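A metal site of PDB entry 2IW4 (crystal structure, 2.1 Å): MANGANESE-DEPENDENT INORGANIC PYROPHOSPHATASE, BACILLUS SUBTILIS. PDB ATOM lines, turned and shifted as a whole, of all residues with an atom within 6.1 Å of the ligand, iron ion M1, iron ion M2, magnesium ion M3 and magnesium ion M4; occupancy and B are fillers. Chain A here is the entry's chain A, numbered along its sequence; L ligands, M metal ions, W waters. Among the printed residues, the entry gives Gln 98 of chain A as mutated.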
ATOM      1  N   HIS A   9       2.895 -15.677  -1.529  1.00  0.00           N
ATOM      2  CA  HIS A   9       1.985 -15.245  -0.478  1.00  0.00           C
ATOM      3  C   HIS A   9       2.095 -13.766  -0.095  1.00  0.00           C
ATOM      4  O   HIS A   9       3.066 -13.072  -0.449  1.00  0.00           O
ATOM      5  CB  HIS A   9       2.142 -16.125   0.772  1.00  0.00           C
ATOM      6  CG  HIS A   9       3.555 -16.333   1.193  1.00  0.00           C
ATOM      7  ND1 HIS A   9       4.265 -15.400   1.931  1.00  0.00           N
ATOM      8  CD2 HIS A   9       4.402 -17.378   0.997  1.00  0.00           C
ATOM      9  CE1 HIS A   9       5.494 -15.865   2.161  1.00  0.00           C
ATOM     10  NE2 HIS A   9       5.583 -17.054   1.602  1.00  0.00           N
ATOM     11  N   ASP A  13       8.248 -13.460   1.308  1.00  0.00           N
ATOM     12  CA  ASP A  13       9.635 -13.733   1.642  1.00  0.00           C
ATOM     13  C   ASP A  13      10.494 -13.929   0.392  1.00  0.00           C
ATOM     14  O   ASP A  13      10.015 -13.766  -0.728  1.00  0.00           O
ATOM     15  CB  ASP A  13       9.772 -14.917   2.597  1.00  0.00           C
ATOM     16  CG  ASP A  13       8.963 -16.092   2.162  1.00  0.00           C
ATOM     17  OD1 ASP A  13       8.524 -16.879   3.035  1.00  0.00           O
ATOM     18  OD2 ASP A  13       8.750 -16.262   0.952  1.00  0.00           O
ATOM     19  N   THR A  14      11.761 -14.266   0.584  1.00  0.00           N
ATOM     20  CA  THR A  14      12.697 -14.380  -0.529  1.00  0.00           C
ATOM     21  C   THR A  14      12.268 -15.494  -1.498  1.00  0.00           C
ATOM     22  O   THR A  14      12.313 -15.317  -2.720  1.00  0.00           O
ATOM     23  CB  THR A  14      14.124 -14.592   0.021  1.00  0.00           C
ATOM     24  OG1 THR A  14      14.435 -13.476   0.873  1.00  0.00           O
ATOM     25  CG2 THR A  14      15.147 -14.677  -1.092  1.00  0.00           C
ATOM     26  N   ASP A  15      11.793 -16.614  -0.963  1.00  0.00           N
ATOM     27  CA  ASP A  15      11.295 -17.709  -1.819  1.00  0.00           C
ATOM     28  C   ASP A  15      10.082 -17.241  -2.636  1.00  0.00           C
ATOM     29  O   ASP A  15      10.051 -17.435  -3.833  1.00  0.00           O
ATOM     30  CB  ASP A  15      10.939 -18.940  -0.976  1.00  0.00           C
ATOM     31  CG  ASP A  15      10.652 -20.187  -1.802  1.00  0.00           C
ATOM     32  OD1 ASP A  15      11.106 -20.308  -2.956  1.00  0.00           O
ATOM     33  OD2 ASP A  15       9.984 -21.115  -1.284  1.00  0.00           O
ATOM     34  N   THR A  16       9.126 -16.572  -1.985  1.00  0.00           N
ATOM     35  CA  THR A  16       7.938 -16.048  -2.669  1.00  0.00           C
ATOM     36  C   THR A  16       8.254 -15.035  -3.811  1.00  0.00           C
ATOM     37  O   THR A  16       7.633 -15.056  -4.901  1.00  0.00           O
ATOM     38  CB  THR A  16       6.933 -15.489  -1.650  1.00  0.00           C
ATOM     39  OG1 THR A  16       5.960 -16.491  -1.339  1.00  0.00           O
ATOM     40  CG2 THR A  16       6.219 -14.321  -2.158  1.00  0.00           C
ATOM     41  N   ASP A  75       4.712 -21.085  -3.824  1.00  0.00           N
ATOM     42  CA  ASP A  75       5.094 -20.958  -2.409  1.00  0.00           C
ATOM     43  C   ASP A  75       3.905 -20.747  -1.458  1.00  0.00           C
ATOM     44  O   ASP A  75       4.079 -20.417  -0.248  1.00  0.00           O
ATOM     45  CB  ASP A  75       6.141 -19.849  -2.248  1.00  0.00           C
ATOM     46  CG  ASP A  75       6.745 -19.808  -0.894  1.00  0.00           C
ATOM     47  OD1 ASP A  75       6.827 -18.701  -0.326  1.00  0.00           O
ATOM     48  OD2 ASP A  75       7.140 -20.892  -0.372  1.00  0.00           O
ATOM     49  N   ASP A  96       4.596 -25.537  -4.985  1.00  0.00           N
ATOM     50  CA  ASP A  96       4.579 -25.173  -3.558  1.00  0.00           C
ATOM     51  C   ASP A  96       5.246 -26.233  -2.673  1.00  0.00           C
ATOM     52  O   ASP A  96       5.632 -27.301  -3.147  1.00  0.00           O
ATOM     53  CB  ASP A  96       3.115 -24.925  -3.130  1.00  0.00           C
ATOM     54  CG  ASP A  96       2.991 -24.327  -1.715  1.00  0.00           C
ATOM     55  OD1 ASP A  96       1.975 -24.562  -1.034  1.00  0.00           O
ATOM     56  OD2 ASP A  96       3.944 -23.671  -1.255  1.00  0.00           O
ATOM     57  N   HIS A  97       5.401 -25.936  -1.376  1.00  0.00           N
ATOM     58  CA  HIS A  97       5.955 -26.901  -0.437  1.00  0.00           C
ATOM     59  C   HIS A  97       5.394 -26.717   0.970  1.00  0.00           C
ATOM     60  O   HIS A  97       6.042 -27.115   1.944  1.00  0.00           O
ATOM     61  CB  HIS A  97       7.497 -26.869  -0.472  1.00  0.00           C
ATOM     62  CG  HIS A  97       8.111 -25.588   0.010  1.00  0.00           C
ATOM     63  ND1 HIS A  97       9.199 -25.568   0.862  1.00  0.00           N
ATOM     64  CD2 HIS A  97       7.831 -24.282  -0.265  1.00  0.00           C
ATOM     65  CE1 HIS A  97       9.534 -24.318   1.120  1.00  0.00           C
ATOM     66  NE2 HIS A  97       8.722 -23.516   0.444  1.00  0.00           N
ATOM     67  N   GLN A  98       4.192 -26.104   1.065  1.00  0.00           N
ATOM     68  CA  GLN A  98       3.451 -25.993   2.316  1.00  0.00           C
ATOM     69  C   GLN A  98       2.426 -27.091   2.403  1.00  0.00           C
ATOM     70  O   GLN A  98       2.128 -27.766   1.406  1.00  0.00           O
ATOM     71  CB  GLN A  98       2.673 -24.663   2.415  1.00  0.00           C
ATOM     72  CG  GLN A  98       3.325 -23.403   1.780  1.00  0.00           C
ATOM     73  CD  GLN A  98       4.650 -23.006   2.387  1.00  0.00           C
ATOM     74  OE1 GLN A  98       4.869 -23.121   3.592  1.00  0.00           O
ATOM     75  NE2 GLN A  98       5.542 -22.488   1.544  1.00  0.00           N
ATOM     76  N   GLY A 117      12.694 -28.376   1.062  1.00  0.00           N
ATOM     77  CA  GLY A 117      12.988 -27.178   1.837  1.00  0.00           C
ATOM     78  C   GLY A 117      12.672 -25.829   1.192  1.00  0.00           C
ATOM     79  O   GLY A 117      12.581 -24.820   1.903  1.00  0.00           O
ATOM     80  N   CYS A 118      12.499 -25.776  -0.131  1.00  0.00           N
ATOM     81  CA  CYS A 118      12.319 -24.489  -0.817  1.00  0.00           C
ATOM     82  C   CYS A 118      11.539 -24.699  -2.118  1.00  0.00           C
ATOM     83  O   CYS A 118      11.773 -25.685  -2.797  1.00  0.00           O
ATOM     84  CB  CYS A 118      13.693 -23.887  -1.128  1.00  0.00           C
ATOM     85  SG  CYS A 118      13.554 -22.251  -1.781  1.00  0.00           S
ATOM     86  N   THR A 119      10.649 -23.770  -2.489  1.00  0.00           N
ATOM     87  CA  THR A 119       9.922 -23.873  -3.756  1.00  0.00           C
ATOM     88  C   THR A 119      10.887 -23.868  -4.941  1.00  0.00           C
ATOM     89  O   THR A 119      10.678 -24.576  -5.935  1.00  0.00           O
ATOM     90  CB  THR A 119       8.954 -22.688  -3.980  1.00  0.00           C
ATOM     91  OG1 THR A 119       8.041 -22.608  -2.878  1.00  0.00           O
ATOM     92  CG2 THR A 119       8.110 -22.859  -5.280  1.00  0.00           C
ATOM     93  N   ALA A 145      16.660 -17.963  -2.387  1.00  0.00           N
ATOM     94  CA  ALA A 145      15.443 -18.582  -1.881  1.00  0.00           C
ATOM     95  C   ALA A 145      15.759 -19.810  -0.996  1.00  0.00           C
ATOM     96  O   ALA A 145      15.242 -19.931   0.117  1.00  0.00           O
ATOM     97  CB  ALA A 145      14.521 -18.952  -3.033  1.00  0.00           C
ATOM     98  N   SER A 148      17.460 -18.814   2.268  1.00  0.00           N
ATOM     99  CA  SER A 148      16.436 -18.173   3.074  1.00  0.00           C
ATOM    100  C   SER A 148      15.540 -19.160   3.778  1.00  0.00           C
ATOM    101  O   SER A 148      15.407 -19.090   4.991  1.00  0.00           O
ATOM    102  CB  SER A 148      15.555 -17.275   2.210  1.00  0.00           C
ATOM    103  OG  SER A 148      14.567 -16.682   3.020  1.00  0.00           O
ATOM    104  N   ASP A 149      14.902 -20.052   3.012  1.00  0.00           N
ATOM    105  CA  ASP A 149      13.996 -21.085   3.558  1.00  0.00           C
ATOM    106  C   ASP A 149      14.680 -22.149   4.391  1.00  0.00           C
ATOM    107  O   ASP A 149      14.077 -22.693   5.308  1.00  0.00           O
ATOM    108  CB  ASP A 149      13.276 -21.804   2.419  1.00  0.00           C
ATOM    109  CG  ASP A 149      12.018 -21.121   2.034  1.00  0.00           C
ATOM    110  OD1 ASP A 149      11.843 -19.959   2.448  1.00  0.00           O
ATOM    111  OD2 ASP A 149      11.174 -21.735   1.360  1.00  0.00           O
ATOM    112  N   THR A 157      13.595 -28.603   7.492  1.00  0.00           N
ATOM    113  CA  THR A 157      12.915 -28.774   6.203  1.00  0.00           C
ATOM    114  C   THR A 157      13.908 -29.048   5.052  1.00  0.00           C
ATOM    115  O   THR A 157      13.503 -29.495   3.980  1.00  0.00           O
ATOM    116  CB  THR A 157      12.119 -27.545   5.816  1.00  0.00           C
ATOM    117  OG1 THR A 157      13.013 -26.429   5.805  1.00  0.00           O
ATOM    118  CG2 THR A 157      11.011 -27.319   6.821  1.00  0.00           C
ATOM    119  N   ASP A 203       6.688 -11.362   8.341  1.00  0.00           N
ATOM    120  CA  ASP A 203       6.615 -12.773   7.994  1.00  0.00           C
ATOM    121  C   ASP A 203       5.424 -13.377   8.739  1.00  0.00           C
ATOM    122  O   ASP A 203       5.544 -14.391   9.467  1.00  0.00           O
ATOM    123  CB  ASP A 203       7.944 -13.442   8.340  1.00  0.00           C
ATOM    124  CG  ASP A 203       8.058 -14.873   7.840  1.00  0.00           C
ATOM    125  OD1 ASP A 203       7.271 -15.293   6.991  1.00  0.00           O
ATOM    126  OD2 ASP A 203       8.982 -15.580   8.301  1.00  0.00           O
ATOM    127  N   LYS A 205       1.599 -15.173   8.680  1.00  0.00           N
ATOM    128  CA  LYS A 205       0.680 -16.029   7.909  1.00  0.00           C
ATOM    129  C   LYS A 205      -0.536 -16.380   8.746  1.00  0.00           C
ATOM    130  O   LYS A 205      -0.409 -16.734   9.906  1.00  0.00           O
ATOM    131  CB  LYS A 205       1.363 -17.319   7.490  1.00  0.00           C
ATOM    132  CG  LYS A 205       2.285 -17.172   6.307  1.00  0.00           C
ATOM    133  CD  LYS A 205       3.031 -18.425   6.048  1.00  0.00           C
ATOM    134  CE  LYS A 205       4.034 -18.262   4.919  1.00  0.00           C
ATOM    135  NZ  LYS A 205       4.498 -19.601   4.402  1.00  0.00           N
ATOM    136  N   PHE A 207      -3.818 -18.918   9.375  1.00  0.00           N
ATOM    137  CA  PHE A 207      -4.189 -20.324   9.268  1.00  0.00           C
ATOM    138  C   PHE A 207      -5.561 -20.491   9.948  1.00  0.00           C
ATOM    139  O   PHE A 207      -5.945 -19.683  10.802  1.00  0.00           O
ATOM    140  CB  PHE A 207      -3.172 -21.216   9.995  1.00  0.00           C
ATOM    141  CG  PHE A 207      -1.817 -21.169   9.394  1.00  0.00           C
ATOM    142  CD1 PHE A 207      -0.843 -20.293   9.889  1.00  0.00           C
ATOM    143  CD2 PHE A 207      -1.517 -21.972   8.310  1.00  0.00           C
ATOM    144  CE1 PHE A 207       0.406 -20.236   9.327  1.00  0.00           C
ATOM    145  CE2 PHE A 207      -0.260 -21.912   7.718  1.00  0.00           C
ATOM    146  CZ  PHE A 207       0.699 -21.033   8.228  1.00  0.00           C
ATOM    147  N   GLN A 218       6.748 -14.891  12.213  1.00  0.00           N
ATOM    148  CA  GLN A 218       8.109 -15.258  12.557  1.00  0.00           C
ATOM    149  C   GLN A 218       9.071 -14.069  12.333  1.00  0.00           C
ATOM    150  O   GLN A 218       8.838 -13.244  11.432  1.00  0.00           O
ATOM    151  CB  GLN A 218       8.573 -16.494  11.749  1.00  0.00           C
ATOM    152  CG  GLN A 218       9.954 -17.012  12.073  1.00  0.00           C
ATOM    153  CD  GLN A 218      10.215 -18.420  11.545  1.00  0.00           C
ATOM    154  OE1 GLN A 218       9.605 -18.853  10.565  1.00  0.00           O
ATOM    155  NE2 GLN A 218      11.142 -19.148  12.183  1.00  0.00           N
ATOM    156  N   SER A 294      11.156 -24.039  12.066  1.00  0.00           N
ATOM    157  CA  SER A 294      10.334 -24.170  10.879  1.00  0.00           C
ATOM    158  C   SER A 294       8.832 -24.114  11.177  1.00  0.00           C
ATOM    159  O   SER A 294       8.350 -24.913  11.985  1.00  0.00           O
ATOM    160  CB  SER A 294      10.636 -25.508  10.206  1.00  0.00           C
ATOM    161  OG  SER A 294       9.580 -25.760   9.288  1.00  0.00           O
ATOM    162  N   ARG A 295       8.106 -23.166  10.568  1.00  0.00           N
ATOM    163  CA  ARG A 295       6.664 -23.031  10.796  1.00  0.00           C
ATOM    164  C   ARG A 295       5.953 -24.244  10.198  1.00  0.00           C
ATOM    165  O   ARG A 295       5.194 -24.912  10.892  1.00  0.00           O
ATOM    166  CB  ARG A 295       6.090 -21.739  10.173  1.00  0.00           C
ATOM    167  CG  ARG A 295       4.589 -21.453  10.484  1.00  0.00           C
ATOM    168  CD  ARG A 295       4.236 -19.968  10.159  1.00  0.00           C
ATOM    169  NE  ARG A 295       5.038 -19.517   9.019  1.00  0.00           N
ATOM    170  CZ  ARG A 295       5.390 -18.255   8.770  1.00  0.00           C
ATOM    171  NH1 ARG A 295       4.966 -17.279   9.565  1.00  0.00           N
ATOM    172  NH2 ARG A 295       6.145 -17.949   7.695  1.00  0.00           N
ATOM    173  N   LYS A 296       6.253 -24.532   8.915  1.00  0.00           N
ATOM    174  CA  LYS A 296       5.556 -25.581   8.167  1.00  0.00           C
ATOM    175  C   LYS A 296       5.707 -26.960   8.777  1.00  0.00           C
ATOM    176  O   LYS A 296       4.812 -27.785   8.640  1.00  0.00           O
ATOM    177  CB  LYS A 296       5.948 -25.638   6.671  1.00  0.00           C
ATOM    178  CG  LYS A 296       7.351 -26.185   6.414  1.00  0.00           C
ATOM    179  CD  LYS A 296       7.689 -26.345   4.933  1.00  0.00           C
ATOM    180  CE  LYS A 296       7.399 -25.063   4.145  1.00  0.00           C
ATOM    181  NZ  LYS A 296       8.406 -23.968   4.362  1.00  0.00           N
ATOM    182  N   LYS A 297       6.855 -27.226   9.424  1.00  0.00           N
ATOM    183  CA  LYS A 297       7.201 -28.568   9.870  1.00  0.00           C
ATOM    184  C   LYS A 297       7.114 -28.692  11.391  1.00  0.00           C
ATOM    185  O   LYS A 297       6.729 -29.729  11.925  1.00  0.00           O
ATOM    186  CB  LYS A 297       8.613 -28.938   9.367  1.00  0.00           C
ATOM    187  CG  LYS A 297       9.170 -30.284   9.936  1.00  0.00           C
ATOM    188  CD  LYS A 297      10.399 -30.751   9.180  1.00  0.00           C
ATOM    189  CE  LYS A 297      10.900 -32.085   9.659  1.00  0.00           C
ATOM    190  NZ  LYS A 297      10.465 -33.092   8.666  1.00  0.00           N
ATOM    191  N   VAL A 300       3.026 -25.568  12.652  1.00  0.00           N
ATOM    192  CA  VAL A 300       1.653 -25.862  12.214  1.00  0.00           C
ATOM    193  C   VAL A 300       1.150 -27.268  12.590  1.00  0.00           C
ATOM    194  O   VAL A 300       0.051 -27.364  13.128  1.00  0.00           O
ATOM    195  CB  VAL A 300       1.370 -25.529  10.700  1.00  0.00           C
ATOM    196  CG1 VAL A 300      -0.024 -26.091  10.271  1.00  0.00           C
ATOM    197  CG2 VAL A 300       1.460 -24.013  10.452  1.00  0.00           C
HETATM  198  P1  LIG L   1       7.809 -20.599   3.694  1.00  0.00           P
HETATM  199  O1  LIG L   1       8.206 -21.689   2.682  1.00  0.00           O
HETATM  200  O2  LIG L   1       9.000 -20.068   4.430  1.00  0.00           O
HETATM  201  O3  LIG L   1       6.817 -19.628   3.096  1.00  0.00           O
HETATM  202  N1  LIG L   1       6.904 -21.380   4.869  1.00  0.00           N
HETATM  203  P2  LIG L   1       6.952 -21.375   6.542  1.00  0.00           P
HETATM  204  O4  LIG L   1       7.588 -22.675   7.101  1.00  0.00           O
HETATM  205  O5  LIG L   1       7.811 -20.198   7.007  1.00  0.00           O
HETATM  206  O6  LIG L   1       5.437 -21.273   6.898  1.00  0.00           O
HETATM  207 FE    FE M   1       7.451 -18.370   1.635  1.00  0.00          FE
HETATM  208 FE    FE M   2       9.065 -21.222   0.705  1.00  0.00          FE
HETATM  209 MG    MG M   3       9.346 -19.104   6.073  1.00  0.00          MG
HETATM  210 MG    MG M   4      10.501 -18.574   3.284  1.00  0.00          MG
HETATM  211  O   HOH W   1      10.005 -23.981   7.362  1.00  0.00           O
HETATM  212  O   HOH W   2       9.597 -18.142   7.965  1.00  0.00           O
HETATM  213  O   HOH W   3      10.816 -22.147   4.758  1.00  0.00           O
HETATM  214  O   HOH W   4      12.143 -17.264   1.799  1.00  0.00           O
HETATM  215  O   HOH W   5       3.583 -23.012   5.982  1.00  0.00           O
HETATM  216  O   HOH W   6       8.198 -17.554   5.673  1.00  0.00           O
HETATM  217  O   HOH W   7       9.319 -21.075   9.061  1.00  0.00           O
HETATM  218  O   HOH W   8      10.664 -20.353   6.868  1.00  0.00           O
HETATM  219  O   HOH W   9      11.081 -18.066   5.357  1.00  0.00           O
HETATM  220  O   HOH W  10       9.386 -19.088   1.564  1.00  0.00           O
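The backbone carbonyl oxygen of Arg 295 is in hydrogen-bond range of the backbone NH of Val 300.
The side-chain hydroxyl (OG1) of Thr 119 lies close to the side-chain carboxylate (OD2) of Asp 15 (2.9 Å).
The side-chain carboxylate of Asp 15 lies within hydrogen-bond range of the side-chain sulfur of Cys 118, at 3.3 Å.
The side-chain carboxylate of Asp 203 lies within salt-bridge range of the guanidinium group of Arg 295, 3.0 Å away.
The side-chain hydroxyl of Thr 16 lies close to the side-chain carboxylate of Asp 75, 2.6 Å away.
OG1 of Thr 16 sits close to N of His 9 (3.2 Å).
N of Gln 98 lies close to OD2 of Asp 96 (3.4 Å).
The side-chain hydroxyl (OG1) of Thr 119 sits close to the side-chain carboxylate (OD2) of Asp 75.
Within 4 Å of magnesium ion M4: Asp 13 and Asp 149.
The nearest printed residue that does not touch magnesium ion M4 is Asp 15 (4.3 Å).
Residues that only touch iron ion M2: Gln 98 and Thr 119.
Six residues have an atom within 4 Å of iron ion M2: Asp 15, Asp 75, His 97, Gln 98, Thr 119 and Asp 149.
Magnesium ion M3 is bound by O2 of the ligand (1.9 Å), water W6 (2.0 Å), water W8 (2.0 Å), O5 of the ligand (2.1 Å), water W2 (2.1 Å) and water W9 (2.1 Å).
Residues that only touch magnesium ion M3: Arg 295 (3.8 Å).
Of the 25 residues printed, 2 come within 4 Å of magnesium ion M3.
The nearest printed residue that does not touch magnesium ion M3 is Asp 203 (4.2 Å).
Iron ion M2 is bound by OD2 of Asp 15 (2.2 Å), O1 of the ligand (2.2 Å), OD2 of Asp 75 (2.2 Å), OD2 of Asp 149 (2.3 Å), water W10 (2.3 Å) and NE2 of His 97 (2.3 Å).
Water W2 lies within hydrogen-bond range of OD2 of Asp 203, OE1 of Gln 218 and NH2 of Arg 295.
Water W6 bridges the side-chain carboxylate of Asp 203 (2.8 Å) and the guanidinium group of Arg 295 (2.9 Å).
Water W4 lies within hydrogen-bond range of the side-chain hydroxyl of Ser 148 (2.8 Å), the backbone NH of Asp 15 (2.9 Å) and the backbone NH of Thr 14 (3.3 Å).
Water W7 lies within hydrogen-bond range of the side-chain amide oxygen (OE1) of Gln 218 (2.7 Å), the backbone NH (N) of Arg 295 (2.8 Å) and an oxygen (O4) of the ligand (3.1 Å).
Water W5 lies within hydrogen-bond range of an oxygen (O6) of the ligand and the side-chain amide oxygen of Gln 98.
Water W3 bridges NZ of Lys 296 (3.0 Å) and O of Asp 149 (3.4 Å).
Thr 16 touches iron ion M1.
Of the 25 residues printed, 4 come within 4 Å of iron ion M1.
An oxygen (O3) of the ligand is bound to iron ion M1 (2.0 Å).
Water W10 is bound to iron ion M1 (2.1 Å).
The side-chain carboxylate (OD1) of Asp 75 binds iron ion M1 (2.1 Å).
NE2 of His 9 is bound to iron ion M1 (2.3 Å).
Iron ion M1 is bound by OD1 of Asp 13, 2.3 Å away.
The side-chain carboxylate (OD2) of Asp 13 is bound to iron ion M1, at 2.6 Å.
OD1 of Asp 149 is bound to magnesium ion M4, at 2.1 Å.
Water W10 is bound to magnesium ion M4 (2.1 Å).
Magnesium ion M4 is bound by water W9, at 2.2 Å.
O2 of the ligand binds magnesium ion M4, 2.4 Å away.
Magnesium ion M4 is bound by water W4.
Magnesium ion M4 has five donor atoms within binding distance.
Slightly farther from magnesium ion M4 lies OD1 of Asp 13 (2.6 Å).
Hydrophobic or aromatic side chains that line the ligand: His 9 and His 97.
Within 4 Å of the ligand: His 9, Asp 13, Asp 75, His 97, Gln 98, Asp 149, Lys 205, Arg 295 and Lys 296.
Along chain A the residues within 4 Å of the ligand span positions 9 to 296.
O4 of the ligand is in salt-bridge range of NZ of Lys 296, at 3.1 Å.
O6 of the ligand lies within salt-bridge range of NE of Arg 295 (2.8 Å).
An oxygen (O6) of the ligand lies within salt-bridge range of the side-chain amino group of Lys 205, at 3.1 Å.
N of Lys 296 sits at hydrogen-bond distance from O4 of the ligand (2.9 Å).
N1 of the ligand sits at hydrogen-bond distance from OE1 of Gln 98 (3.0 Å).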
